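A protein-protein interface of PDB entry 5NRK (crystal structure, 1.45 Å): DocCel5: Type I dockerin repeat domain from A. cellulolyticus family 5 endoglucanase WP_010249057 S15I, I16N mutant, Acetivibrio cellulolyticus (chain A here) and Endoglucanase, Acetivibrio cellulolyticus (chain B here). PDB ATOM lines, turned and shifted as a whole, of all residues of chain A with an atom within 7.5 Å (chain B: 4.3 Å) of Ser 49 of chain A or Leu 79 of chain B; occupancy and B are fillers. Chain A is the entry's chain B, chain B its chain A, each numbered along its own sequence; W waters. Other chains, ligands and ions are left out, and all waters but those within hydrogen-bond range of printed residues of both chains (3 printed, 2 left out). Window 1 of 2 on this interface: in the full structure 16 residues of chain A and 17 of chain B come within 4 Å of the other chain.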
ATOM      1  N   MET A  19      -4.420 -13.576  22.203  1.00  0.00           N
ATOM      2  CA  MET A  19      -5.661 -13.037  21.642  1.00  0.00           C
ATOM      3  C   MET A  19      -6.478 -14.139  20.956  1.00  0.00           C
ATOM      4  O   MET A  19      -7.699 -14.205  21.128  1.00  0.00           O
ATOM      5  CB  MET A  19      -5.370 -11.870  20.718  1.00  0.00           C
ATOM      6  CG  MET A  19      -6.557 -11.389  19.908  1.00  0.00           C
ATOM      7  SD  MET A  19      -7.593 -10.357  20.925  1.00  0.00           S
ATOM      8  CE  MET A  19      -6.585  -8.854  21.073  1.00  0.00           C
ATOM      9  N   ARG A  20      -5.810 -15.001  20.179  1.00  0.00           N
ATOM     10  CA  ARG A  20      -6.514 -16.082  19.515  1.00  0.00           C
ATOM     11  C   ARG A  20      -7.168 -16.989  20.547  1.00  0.00           C
ATOM     12  O   ARG A  20      -8.345 -17.352  20.443  1.00  0.00           O
ATOM     13  CB  ARG A  20      -5.571 -16.904  18.623  1.00  0.00           C
ATOM     14  CG  ARG A  20      -6.341 -17.865  17.742  1.00  0.00           C
ATOM     15  CD  ARG A  20      -5.467 -18.582  16.722  1.00  0.00           C
ATOM     16  NE  ARG A  20      -6.335 -19.254  15.737  1.00  0.00           N
ATOM     17  CZ  ARG A  20      -6.764 -20.489  15.808  1.00  0.00           C
ATOM     18  NH1 ARG A  20      -6.403 -21.286  16.814  1.00  0.00           N
ATOM     19  NH2 ARG A  20      -7.586 -20.943  14.872  1.00  0.00           N
ATOM     20  N   ASN A  21      -6.411 -17.364  21.567  1.00  0.00           N
ATOM     21  CA  ASN A  21      -6.921 -18.208  22.635  1.00  0.00           C
ATOM     22  C   ASN A  21      -8.060 -17.586  23.404  1.00  0.00           C
ATOM     23  O   ASN A  21      -9.038 -18.272  23.741  1.00  0.00           O
ATOM     24  CB  ASN A  21      -5.803 -18.706  23.545  1.00  0.00           C
ATOM     25  CG  ASN A  21      -5.011 -19.829  22.885  1.00  0.00           C
ATOM     26  OD1 ASN A  21      -5.608 -20.851  22.507  1.00  0.00           O
ATOM     27  ND2 ASN A  21      -3.686 -19.698  22.772  1.00  0.00           N
ATOM     28  N   TYR A  22      -7.987 -16.278  23.645  1.00  0.00           N
ATOM     29  CA  TYR A  22      -9.078 -15.570  24.289  1.00  0.00           C
ATOM     30  C   TYR A  22     -10.356 -15.643  23.449  1.00  0.00           C
ATOM     31  O   TYR A  22     -11.438 -15.959  23.959  1.00  0.00           O
ATOM     32  CB  TYR A  22      -8.670 -14.113  24.488  1.00  0.00           C
ATOM     33  CG  TYR A  22      -9.749 -13.240  25.026  1.00  0.00           C
ATOM     34  CD1 TYR A  22     -10.114 -13.305  26.356  1.00  0.00           C
ATOM     35  CD2 TYR A  22     -10.431 -12.358  24.188  1.00  0.00           C
ATOM     36  CE1 TYR A  22     -11.125 -12.496  26.850  1.00  0.00           C
ATOM     37  CE2 TYR A  22     -11.448 -11.547  24.660  1.00  0.00           C
ATOM     38  CZ  TYR A  22     -11.779 -11.623  26.000  1.00  0.00           C
ATOM     39  OH  TYR A  22     -12.789 -10.814  26.489  1.00  0.00           O
ATOM     40  N   LEU A  23     -10.224 -15.386  22.149  1.00  0.00           N
ATOM     41  CA  LEU A  23     -11.396 -15.396  21.261  1.00  0.00           C
ATOM     42  C   LEU A  23     -11.964 -16.793  21.041  1.00  0.00           C
ATOM     43  O   LEU A  23     -13.148 -16.924  20.738  1.00  0.00           O
ATOM     44  CB  LEU A  23     -11.067 -14.706  19.938  1.00  0.00           C
ATOM     45  CG  LEU A  23     -10.741 -13.218  20.049  1.00  0.00           C
ATOM     46  CD1 LEU A  23     -10.277 -12.688  18.710  1.00  0.00           C
ATOM     47  CD2 LEU A  23     -11.910 -12.410  20.569  1.00  0.00           C
ATOM     48  N   LEU A  24     -11.179 -17.829  21.302  1.00  0.00           N
ATOM     49  CA  LEU A  24     -11.662 -19.199  21.257  1.00  0.00           C
ATOM     50  C   LEU A  24     -12.156 -19.742  22.602  1.00  0.00           C
ATOM     51  O   LEU A  24     -12.572 -20.885  22.699  1.00  0.00           O
ATOM     52  CB  LEU A  24     -10.571 -20.121  20.698  1.00  0.00           C
ATOM     53  CG  LEU A  24     -10.350 -19.933  19.192  1.00  0.00           C
ATOM     54  CD1 LEU A  24      -9.098 -20.665  18.768  1.00  0.00           C
ATOM     55  CD2 LEU A  24     -11.545 -20.416  18.385  1.00  0.00           C
ATOM     56  N   ASN A  42      -8.793  -0.722  18.326  1.00  0.00           N
ATOM     57  CA  ASN A  42      -9.533   0.270  17.518  1.00  0.00           C
ATOM     58  C   ASN A  42     -10.415   1.213  18.319  1.00  0.00           C
ATOM     59  O   ASN A  42     -11.089   2.049  17.732  1.00  0.00           O
ATOM     60  CB  ASN A  42     -10.324  -0.425  16.403  1.00  0.00           C
ATOM     61  CG  ASN A  42     -11.270  -1.475  16.920  1.00  0.00           C
ATOM     62  OD1 ASN A  42     -11.484  -1.564  18.117  1.00  0.00           O
ATOM     63  ND2 ASN A  42     -11.849  -2.278  16.025  1.00  0.00           N
ATOM     64  N   SER A  46     -14.367  -2.852  22.993  1.00  0.00           N
ATOM     65  CA  SER A  46     -14.624  -4.294  22.909  1.00  0.00           C
ATOM     66  C   SER A  46     -13.340  -4.970  22.440  1.00  0.00           C
ATOM     67  O   SER A  46     -12.553  -4.370  21.704  1.00  0.00           O
ATOM     68  CB  SER A  46     -15.730  -4.630  21.886  1.00  0.00           C
ATOM     69  OG  SER A  46     -17.025  -4.179  22.255  1.00  0.00           O
ATOM     70  N   ILE A  47     -13.132  -6.214  22.841  1.00  0.00           N
ATOM     71  CA  ILE A  47     -12.043  -7.023  22.340  1.00  0.00           C
ATOM     72  C   ILE A  47     -12.650  -8.107  21.476  1.00  0.00           C
ATOM     73  O   ILE A  47     -13.349  -9.001  21.994  1.00  0.00           O
ATOM     74  CB  ILE A  47     -11.219  -7.684  23.461  1.00  0.00           C
ATOM     75  CG1 ILE A  47     -10.666  -6.625  24.436  1.00  0.00           C
ATOM     76  CG2 ILE A  47     -10.081  -8.489  22.863  1.00  0.00           C
ATOM     77  CD1 ILE A  47     -10.034  -7.233  25.665  1.00  0.00           C
ATOM     78  N   ASN A  48     -12.410  -8.043  20.170  1.00  0.00           N
ATOM     79  CA  ASN A  48     -13.021  -9.027  19.271  1.00  0.00           C
ATOM     80  C   ASN A  48     -12.156  -9.243  18.051  1.00  0.00           C
ATOM     81  O   ASN A  48     -10.982  -8.852  18.039  1.00  0.00           O
ATOM     82  CB  ASN A  48     -14.461  -8.613  18.936  1.00  0.00           C
ATOM     83  CG  ASN A  48     -14.554  -7.290  18.211  1.00  0.00           C
ATOM     84  OD1 ASN A  48     -13.662  -6.924  17.450  1.00  0.00           O
ATOM     85  ND2 ASN A  48     -15.657  -6.572  18.435  1.00  0.00           N
ATOM     86  N   SER A  49     -12.691  -9.909  17.035  1.00  0.00           N
ATOM     87  CA  SER A  49     -11.875 -10.294  15.897  1.00  0.00           C
ATOM     88  C   SER A  49     -11.332  -9.128  15.085  1.00  0.00           C
ATOM     89  O   SER A  49     -10.344  -9.285  14.377  1.00  0.00           O
ATOM     90  CB  SER A  49     -12.607 -11.310  15.008  1.00  0.00           C
ATOM     91  OG  SER A  49     -13.803 -10.781  14.487  1.00  0.00           O
ATOM     92  N   LEU A  50     -11.936  -7.943  15.191  1.00  0.00           N
ATOM     93  CA  LEU A  50     -11.351  -6.757  14.571  1.00  0.00           C
ATOM     94  C   LEU A  50     -10.007  -6.420  15.210  1.00  0.00           C
ATOM     95  O   LEU A  50      -9.032  -6.065  14.528  1.00  0.00           O
ATOM     96  CB  LEU A  50     -12.271  -5.537  14.699  1.00  0.00           C
ATOM     97  CG  LEU A  50     -13.659  -5.594  14.086  1.00  0.00           C
ATOM     98  CD1 LEU A  50     -14.397  -4.289  14.266  1.00  0.00           C
ATOM     99  CD2 LEU A  50     -13.541  -5.909  12.629  1.00  0.00           C
ATOM    100  N   ASP A  51      -9.942  -6.538  16.526  1.00  0.00           N
ATOM    101  CA  ASP A  51      -8.672  -6.310  17.237  1.00  0.00           C
ATOM    102  C   ASP A  51      -7.627  -7.354  16.861  1.00  0.00           C
ATOM    103  O   ASP A  51      -6.442  -7.031  16.681  1.00  0.00           O
ATOM    104  CB  ASP A  51      -8.925  -6.290  18.731  1.00  0.00           C
ATOM    105  CG  ASP A  51      -9.963  -5.276  19.087  1.00  0.00           C
ATOM    106  OD1 ASP A  51      -9.690  -4.055  18.969  1.00  0.00           O
ATOM    107  OD2 ASP A  51     -11.094  -5.650  19.457  1.00  0.00           O
ATOM    108  N   PHE A  52      -8.050  -8.607  16.717  1.00  0.00           N
ATOM    109  CA  PHE A  52      -7.180  -9.691  16.277  1.00  0.00           C
ATOM    110  C   PHE A  52      -6.564  -9.385  14.901  1.00  0.00           C
ATOM    111  O   PHE A  52      -5.367  -9.572  14.688  1.00  0.00           O
ATOM    112  CB  PHE A  52      -8.022 -10.973  16.317  1.00  0.00           C
ATOM    113  CG  PHE A  52      -7.285 -12.262  16.072  1.00  0.00           C
ATOM    114  CD1 PHE A  52      -6.146 -12.612  16.793  1.00  0.00           C
ATOM    115  CD2 PHE A  52      -7.790 -13.167  15.162  1.00  0.00           C
ATOM    116  CE1 PHE A  52      -5.550 -13.844  16.586  1.00  0.00           C
ATOM    117  CE2 PHE A  52      -7.182 -14.393  14.950  1.00  0.00           C
ATOM    118  CZ  PHE A  52      -6.039 -14.707  15.635  1.00  0.00           C
ATOM    119  N   ALA A  53      -7.398  -8.886  13.995  1.00  0.00           N
ATOM    120  CA  ALA A  53      -6.947  -8.510  12.676  1.00  0.00           C
ATOM    121  C   ALA A  53      -5.945  -7.380  12.723  1.00  0.00           C
ATOM    122  O   ALA A  53      -4.951  -7.393  11.988  1.00  0.00           O
ATOM    123  CB  ALA A  53      -8.140  -8.097  11.819  1.00  0.00           C
ATOM    124  N   ILE A  54      -6.195  -6.388  13.573  1.00  0.00           N
ATOM    125  CA  ILE A  54      -5.297  -5.260  13.689  1.00  0.00           C
ATOM    126  C   ILE A  54      -3.936  -5.711  14.223  1.00  0.00           C
ATOM    127  O   ILE A  54      -2.877  -5.288  13.735  1.00  0.00           O
ATOM    128  CB  ILE A  54      -5.914  -4.155  14.569  1.00  0.00           C
ATOM    129  CG1 ILE A  54      -7.118  -3.545  13.855  1.00  0.00           C
ATOM    130  CG2 ILE A  54      -4.878  -3.085  14.904  1.00  0.00           C
ATOM    131  CD1 ILE A  54      -8.031  -2.737  14.756  1.00  0.00           C
ATOM    132  N   MET A  55      -3.950  -6.589  15.209  1.00  0.00           N
ATOM    133  CA  MET A  55      -2.709  -7.140  15.725  1.00  0.00           C
ATOM    134  C   MET A  55      -1.944  -7.897  14.630  1.00  0.00           C
ATOM    135  O   MET A  55      -0.715  -7.784  14.528  1.00  0.00           O
ATOM    136  CB  MET A  55      -3.013  -8.063  16.895  1.00  0.00           C
ATOM    137  CG  MET A  55      -1.733  -8.609  17.492  1.00  0.00           C
ATOM    138  SD  MET A  55      -1.913  -9.568  18.989  1.00  0.00           S
ATOM    139  CE  MET A  55      -2.643  -8.500  20.219  1.00  0.00           C
ATOM    140  N   THR B  36     -13.069 -10.738   9.035  1.00  0.00           N
ATOM    141  CA  THR B  36     -12.935 -11.215  10.392  1.00  0.00           C
ATOM    142  C   THR B  36     -14.306 -11.641  10.818  1.00  0.00           C
ATOM    143  O   THR B  36     -15.270 -11.081  10.380  1.00  0.00           O
ATOM    144  CB  THR B  36     -12.394 -10.129  11.400  1.00  0.00           C
ATOM    145  OG1 THR B  36     -13.466  -9.363  11.971  1.00  0.00           O
ATOM    146  CG2 THR B  36     -11.475  -9.169  10.752  1.00  0.00           C
ATOM    147  N   ALA B  37     -14.321 -12.612  11.720  1.00  0.00           N
ATOM    148  CA  ALA B  37     -15.573 -12.954  12.397  1.00  0.00           C
ATOM    149  C   ALA B  37     -15.283 -13.575  13.736  1.00  0.00           C
ATOM    150  O   ALA B  37     -14.314 -14.308  13.894  1.00  0.00           O
ATOM    151  CB  ALA B  37     -16.397 -13.926  11.585  1.00  0.00           C
ATOM    152  N   ASP B  38     -16.136 -13.305  14.718  1.00  0.00           N
ATOM    153  CA  ASP B  38     -16.095 -14.072  15.956  1.00  0.00           C
ATOM    154  C   ASP B  38     -17.486 -14.083  16.546  1.00  0.00           C
ATOM    155  O   ASP B  38     -18.168 -13.048  16.577  1.00  0.00           O
ATOM    156  CB  ASP B  38     -15.060 -13.556  16.965  1.00  0.00           C
ATOM    157  CG  ASP B  38     -15.378 -12.185  17.505  1.00  0.00           C
ATOM    158  OD1 ASP B  38     -15.166 -11.178  16.800  1.00  0.00           O
ATOM    159  OD2 ASP B  38     -15.801 -12.096  18.693  1.00  0.00           O
ATOM    160  N   ASN B  65      -6.945 -19.781   8.669  1.00  0.00           N
ATOM    161  CA  ASN B  65      -7.844 -18.656   8.930  1.00  0.00           C
ATOM    162  C   ASN B  65      -9.008 -18.962   9.860  1.00  0.00           C
ATOM    163  O   ASN B  65      -9.566 -18.044  10.465  1.00  0.00           O
ATOM    164  CB  ASN B  65      -8.427 -18.144   7.624  1.00  0.00           C
ATOM    165  CG  ASN B  65      -7.415 -17.452   6.748  1.00  0.00           C
ATOM    166  OD1 ASN B  65      -6.275 -17.202   7.151  1.00  0.00           O
ATOM    167  ND2 ASN B  65      -7.839 -17.099   5.542  1.00  0.00           N
ATOM    168  N   PHE B  66      -9.366 -20.235  10.014  1.00  0.00           N
ATOM    169  CA  PHE B  66     -10.563 -20.634  10.758  1.00  0.00           C
ATOM    170  C   PHE B  66     -10.201 -21.363  12.021  1.00  0.00           C
ATOM    171  O   PHE B  66      -9.293 -22.191  12.035  1.00  0.00           O
ATOM    172  CB  PHE B  66     -11.410 -21.544   9.862  1.00  0.00           C
ATOM    173  CG  PHE B  66     -12.716 -21.973  10.470  1.00  0.00           C
ATOM    174  CD1 PHE B  66     -13.852 -21.201  10.317  1.00  0.00           C
ATOM    175  CD2 PHE B  66     -12.805 -23.175  11.171  1.00  0.00           C
ATOM    176  CE1 PHE B  66     -15.051 -21.624  10.865  1.00  0.00           C
ATOM    177  CE2 PHE B  66     -13.999 -23.580  11.736  1.00  0.00           C
ATOM    178  CZ  PHE B  66     -15.115 -22.785  11.586  1.00  0.00           C
ATOM    179  N   GLY B  67     -10.958 -21.078  13.078  1.00  0.00           N
ATOM    180  CA  GLY B  67     -10.857 -21.839  14.311  1.00  0.00           C
ATOM    181  C   GLY B  67     -12.213 -21.996  14.973  1.00  0.00           C
ATOM    182  O   GLY B  67     -13.078 -21.141  14.858  1.00  0.00           O
ATOM    183  N   VAL B  78     -16.345 -19.437  17.751  1.00  0.00           N
ATOM    184  CA  VAL B  78     -15.982 -19.547  16.341  1.00  0.00           C
ATOM    185  C   VAL B  78     -15.192 -18.311  15.964  1.00  0.00           C
ATOM    186  O   VAL B  78     -15.505 -17.203  16.406  1.00  0.00           O
ATOM    187  CB  VAL B  78     -17.244 -19.648  15.467  1.00  0.00           C
ATOM    188  CG1 VAL B  78     -16.870 -19.903  14.014  1.00  0.00           C
ATOM    189  CG2 VAL B  78     -18.173 -20.751  15.971  1.00  0.00           C
ATOM    190  N   LEU B  79     -14.160 -18.491  15.145  1.00  0.00           N
ATOM    191  CA  LEU B  79     -13.218 -17.409  14.823  1.00  0.00           C
ATOM    192  C   LEU B  79     -12.757 -17.529  13.393  1.00  0.00           C
ATOM    193  O   LEU B  79     -12.379 -18.608  12.944  1.00  0.00           O
ATOM    194  CB  LEU B  79     -11.997 -17.487  15.759  1.00  0.00           C
ATOM    195  CG  LEU B  79     -10.915 -16.433  15.538  1.00  0.00           C
ATOM    196  CD1 LEU B  79     -11.416 -15.028  15.792  1.00  0.00           C
ATOM    197  CD2 LEU B  79      -9.750 -16.749  16.468  1.00  0.00           C
ATOM    198  N   PHE B  80     -12.781 -16.413  12.670  1.00  0.00           N
ATOM    199  CA  PHE B  80     -12.213 -16.343  11.343  1.00  0.00           C
ATOM    200  C   PHE B  80     -11.402 -15.072  11.216  1.00  0.00           C
ATOM    201  O   PHE B  80     -11.814 -13.991  11.661  1.00  0.00           O
ATOM    202  CB  PHE B  80     -13.299 -16.356  10.247  1.00  0.00           C
ATOM    203  CG  PHE B  80     -12.767 -16.054   8.870  1.00  0.00           C
ATOM    204  CD1 PHE B  80     -12.094 -17.009   8.135  1.00  0.00           C
ATOM    205  CD2 PHE B  80     -12.901 -14.782   8.322  1.00  0.00           C
ATOM    206  CE1 PHE B  80     -11.565 -16.720   6.894  1.00  0.00           C
ATOM    207  CE2 PHE B  80     -12.353 -14.483   7.089  1.00  0.00           C
ATOM    208  CZ  PHE B  80     -11.693 -15.445   6.371  1.00  0.00           C
ATOM    209  N   THR B 122     -19.844 -10.736  15.739  1.00  0.00           N
ATOM    210  CA  THR B 122     -18.993  -9.716  15.177  1.00  0.00           C
ATOM    211  C   THR B 122     -18.453 -10.157  13.820  1.00  0.00           C
ATOM    212  O   THR B 122     -17.932 -11.265  13.679  1.00  0.00           O
ATOM    213  CB  THR B 122     -17.811  -9.435  16.110  1.00  0.00           C
ATOM    214  OG1 THR B 122     -18.305  -8.879  17.329  1.00  0.00           O
ATOM    215  CG2 THR B 122     -16.834  -8.496  15.489  1.00  0.00           C
HETATM  216  O   HOH W   1     -15.279 -16.388  19.113  1.00  0.00           O
HETATM  217  O   HOH W   2      -7.725 -18.808  12.873  1.00  0.00           O
HETATM  218  O   HOH W   3     -15.110 -11.173  21.466  1.00  0.00           O
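N of Asp 38 of chain B lies within hydrogen-bond range of O of Thr 122 of chain B (2.9 Å). N of Ala 37 of chain B lies within hydrogen-bond range of O of Phe 80 of chain B. The side-chain amide oxygen (OD1) of Asn 48 of chain A lies within hydrogen-bond range of the backbone NH (N) of Leu 50 of chain A (3.0 Å). The backbone carbonyl oxygen (O) of Leu 79 of chain B is in hydrogen-bond range of the backbone NH (N) of Gly 67 of chain B. N of Asn 48 of chain A sits close to OD2 of Asp 51 of chain A, 2.8 Å away.
Of the 17 printed residues of chain A, 8 touch a printed residue of chain B. Hydrophobic or aromatic side chains of chain A within 4 Å of the printed part of chain B: Leu 23, Leu 24, Leu 50, Phe 52 and Ala 53. Of the 10 printed residues of chain B, 7 touch a printed residue of chain A. Hydrophobic or aromatic side chains of chain B within 4 Å of the printed part of chain A: Leu 79. Among the printed residues, 16 pairs touch across the chains. Among the printed residues, no Asp or Glu carboxylate lies within 4 Å of a Lys or Arg side-chain nitrogen of the other chain.
Among the printed residues, merely in contact across the chains: Asn 48 of chain A with Asp 38 of chain B (3.4 Å), Arg 20 of chain A with Gly 67 of chain B (3.4 Å), Leu 50 of chain A with Thr 36 of chain B (3.5 Å), Arg 20 of chain A with Phe 66 of chain B (3.5 Å), Ala 53 of chain A with Thr 36 of chain B (3.7 Å), Asn 48 of chain A with Thr 122 of chain B (3.7 Å), Phe 52 of chain A with Leu 79 of chain B (3.8 Å), Arg 20 of chain A with Leu 79 of chain B (3.8 Å), Leu 24 of chain A with Gly 67 of chain B (3.8 Å), Leu 23 of chain A with Leu 79 of chain B (3.9 Å), Ser 49 of chain A with Thr 122 of chain B (3.9 Å), Leu 24 of chain A with Leu 79 of chain B (3.96 Å) and Ser 49 of chain A with Leu 79 of chain B (3.98 Å).
The side-chain carboxylate of Asp 38 of chain B sits at hydrogen-bond distance from the side-chain hydroxyl of Ser 49 of chain A, 2.7 Å away. The backbone NH (N) of Ala 37 of chain B lies close to the side-chain hydroxyl (OG) of Ser 49 of chain A (3.4 Å). The side-chain hydroxyl of Thr 36 of chain B sits at hydrogen-bond distance from the side-chain hydroxyl of Ser 49 of chain A (2.9 Å).
Water W1 lies within hydrogen-bond range of the backbone carbonyl oxygen of Leu 23 of chain A (2.7 Å) and the backbone carbonyl oxygen of Val 78 of chain B (2.8 Å). Water W3 bridges O of Ile 47 of chain A and OD2 of Asp 38 of chain B. Water W2 bridges NH2 of Arg 20 of chain A (2.9 Å) and O of Asn 65 of chain B (3.1 Å).
Of the printed residues of chain B, Arg 20 of chain A touches Phe 66, Gly 67 and Leu 79. Of the printed residues of chain B, Asn 48 of chain A touches Asp 38 and Thr 122. Printed residues of chain B within 4 Å of Ser 49 of chain A: Thr 36, Ala 37, Asp 38, Leu 79 and Thr 122. Printed residues of chain B within 4 Å of Leu 50 of chain A: Thr 36 (3.5 Å). Of the printed residues of chain B, Phe 52 of chain A touches Leu 79. Printed residues of chain A within 4 Å of Leu 79 of chain B: Arg 20, Leu 23, Leu 24, Ser 49 and Phe 52. Of the printed residues of chain A, Thr 122 of chain B touches Asn 48 (3.7 Å) and Ser 49 (3.9 Å). The nearest printed residue of chain B that does not touch Ser 49 of chain A is Phe 80 of chain B (4.4 Å). The nearest printed residue of chain A that does not touch Ala 37 of chain B is Leu 50 of chain A (6.3 Å).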
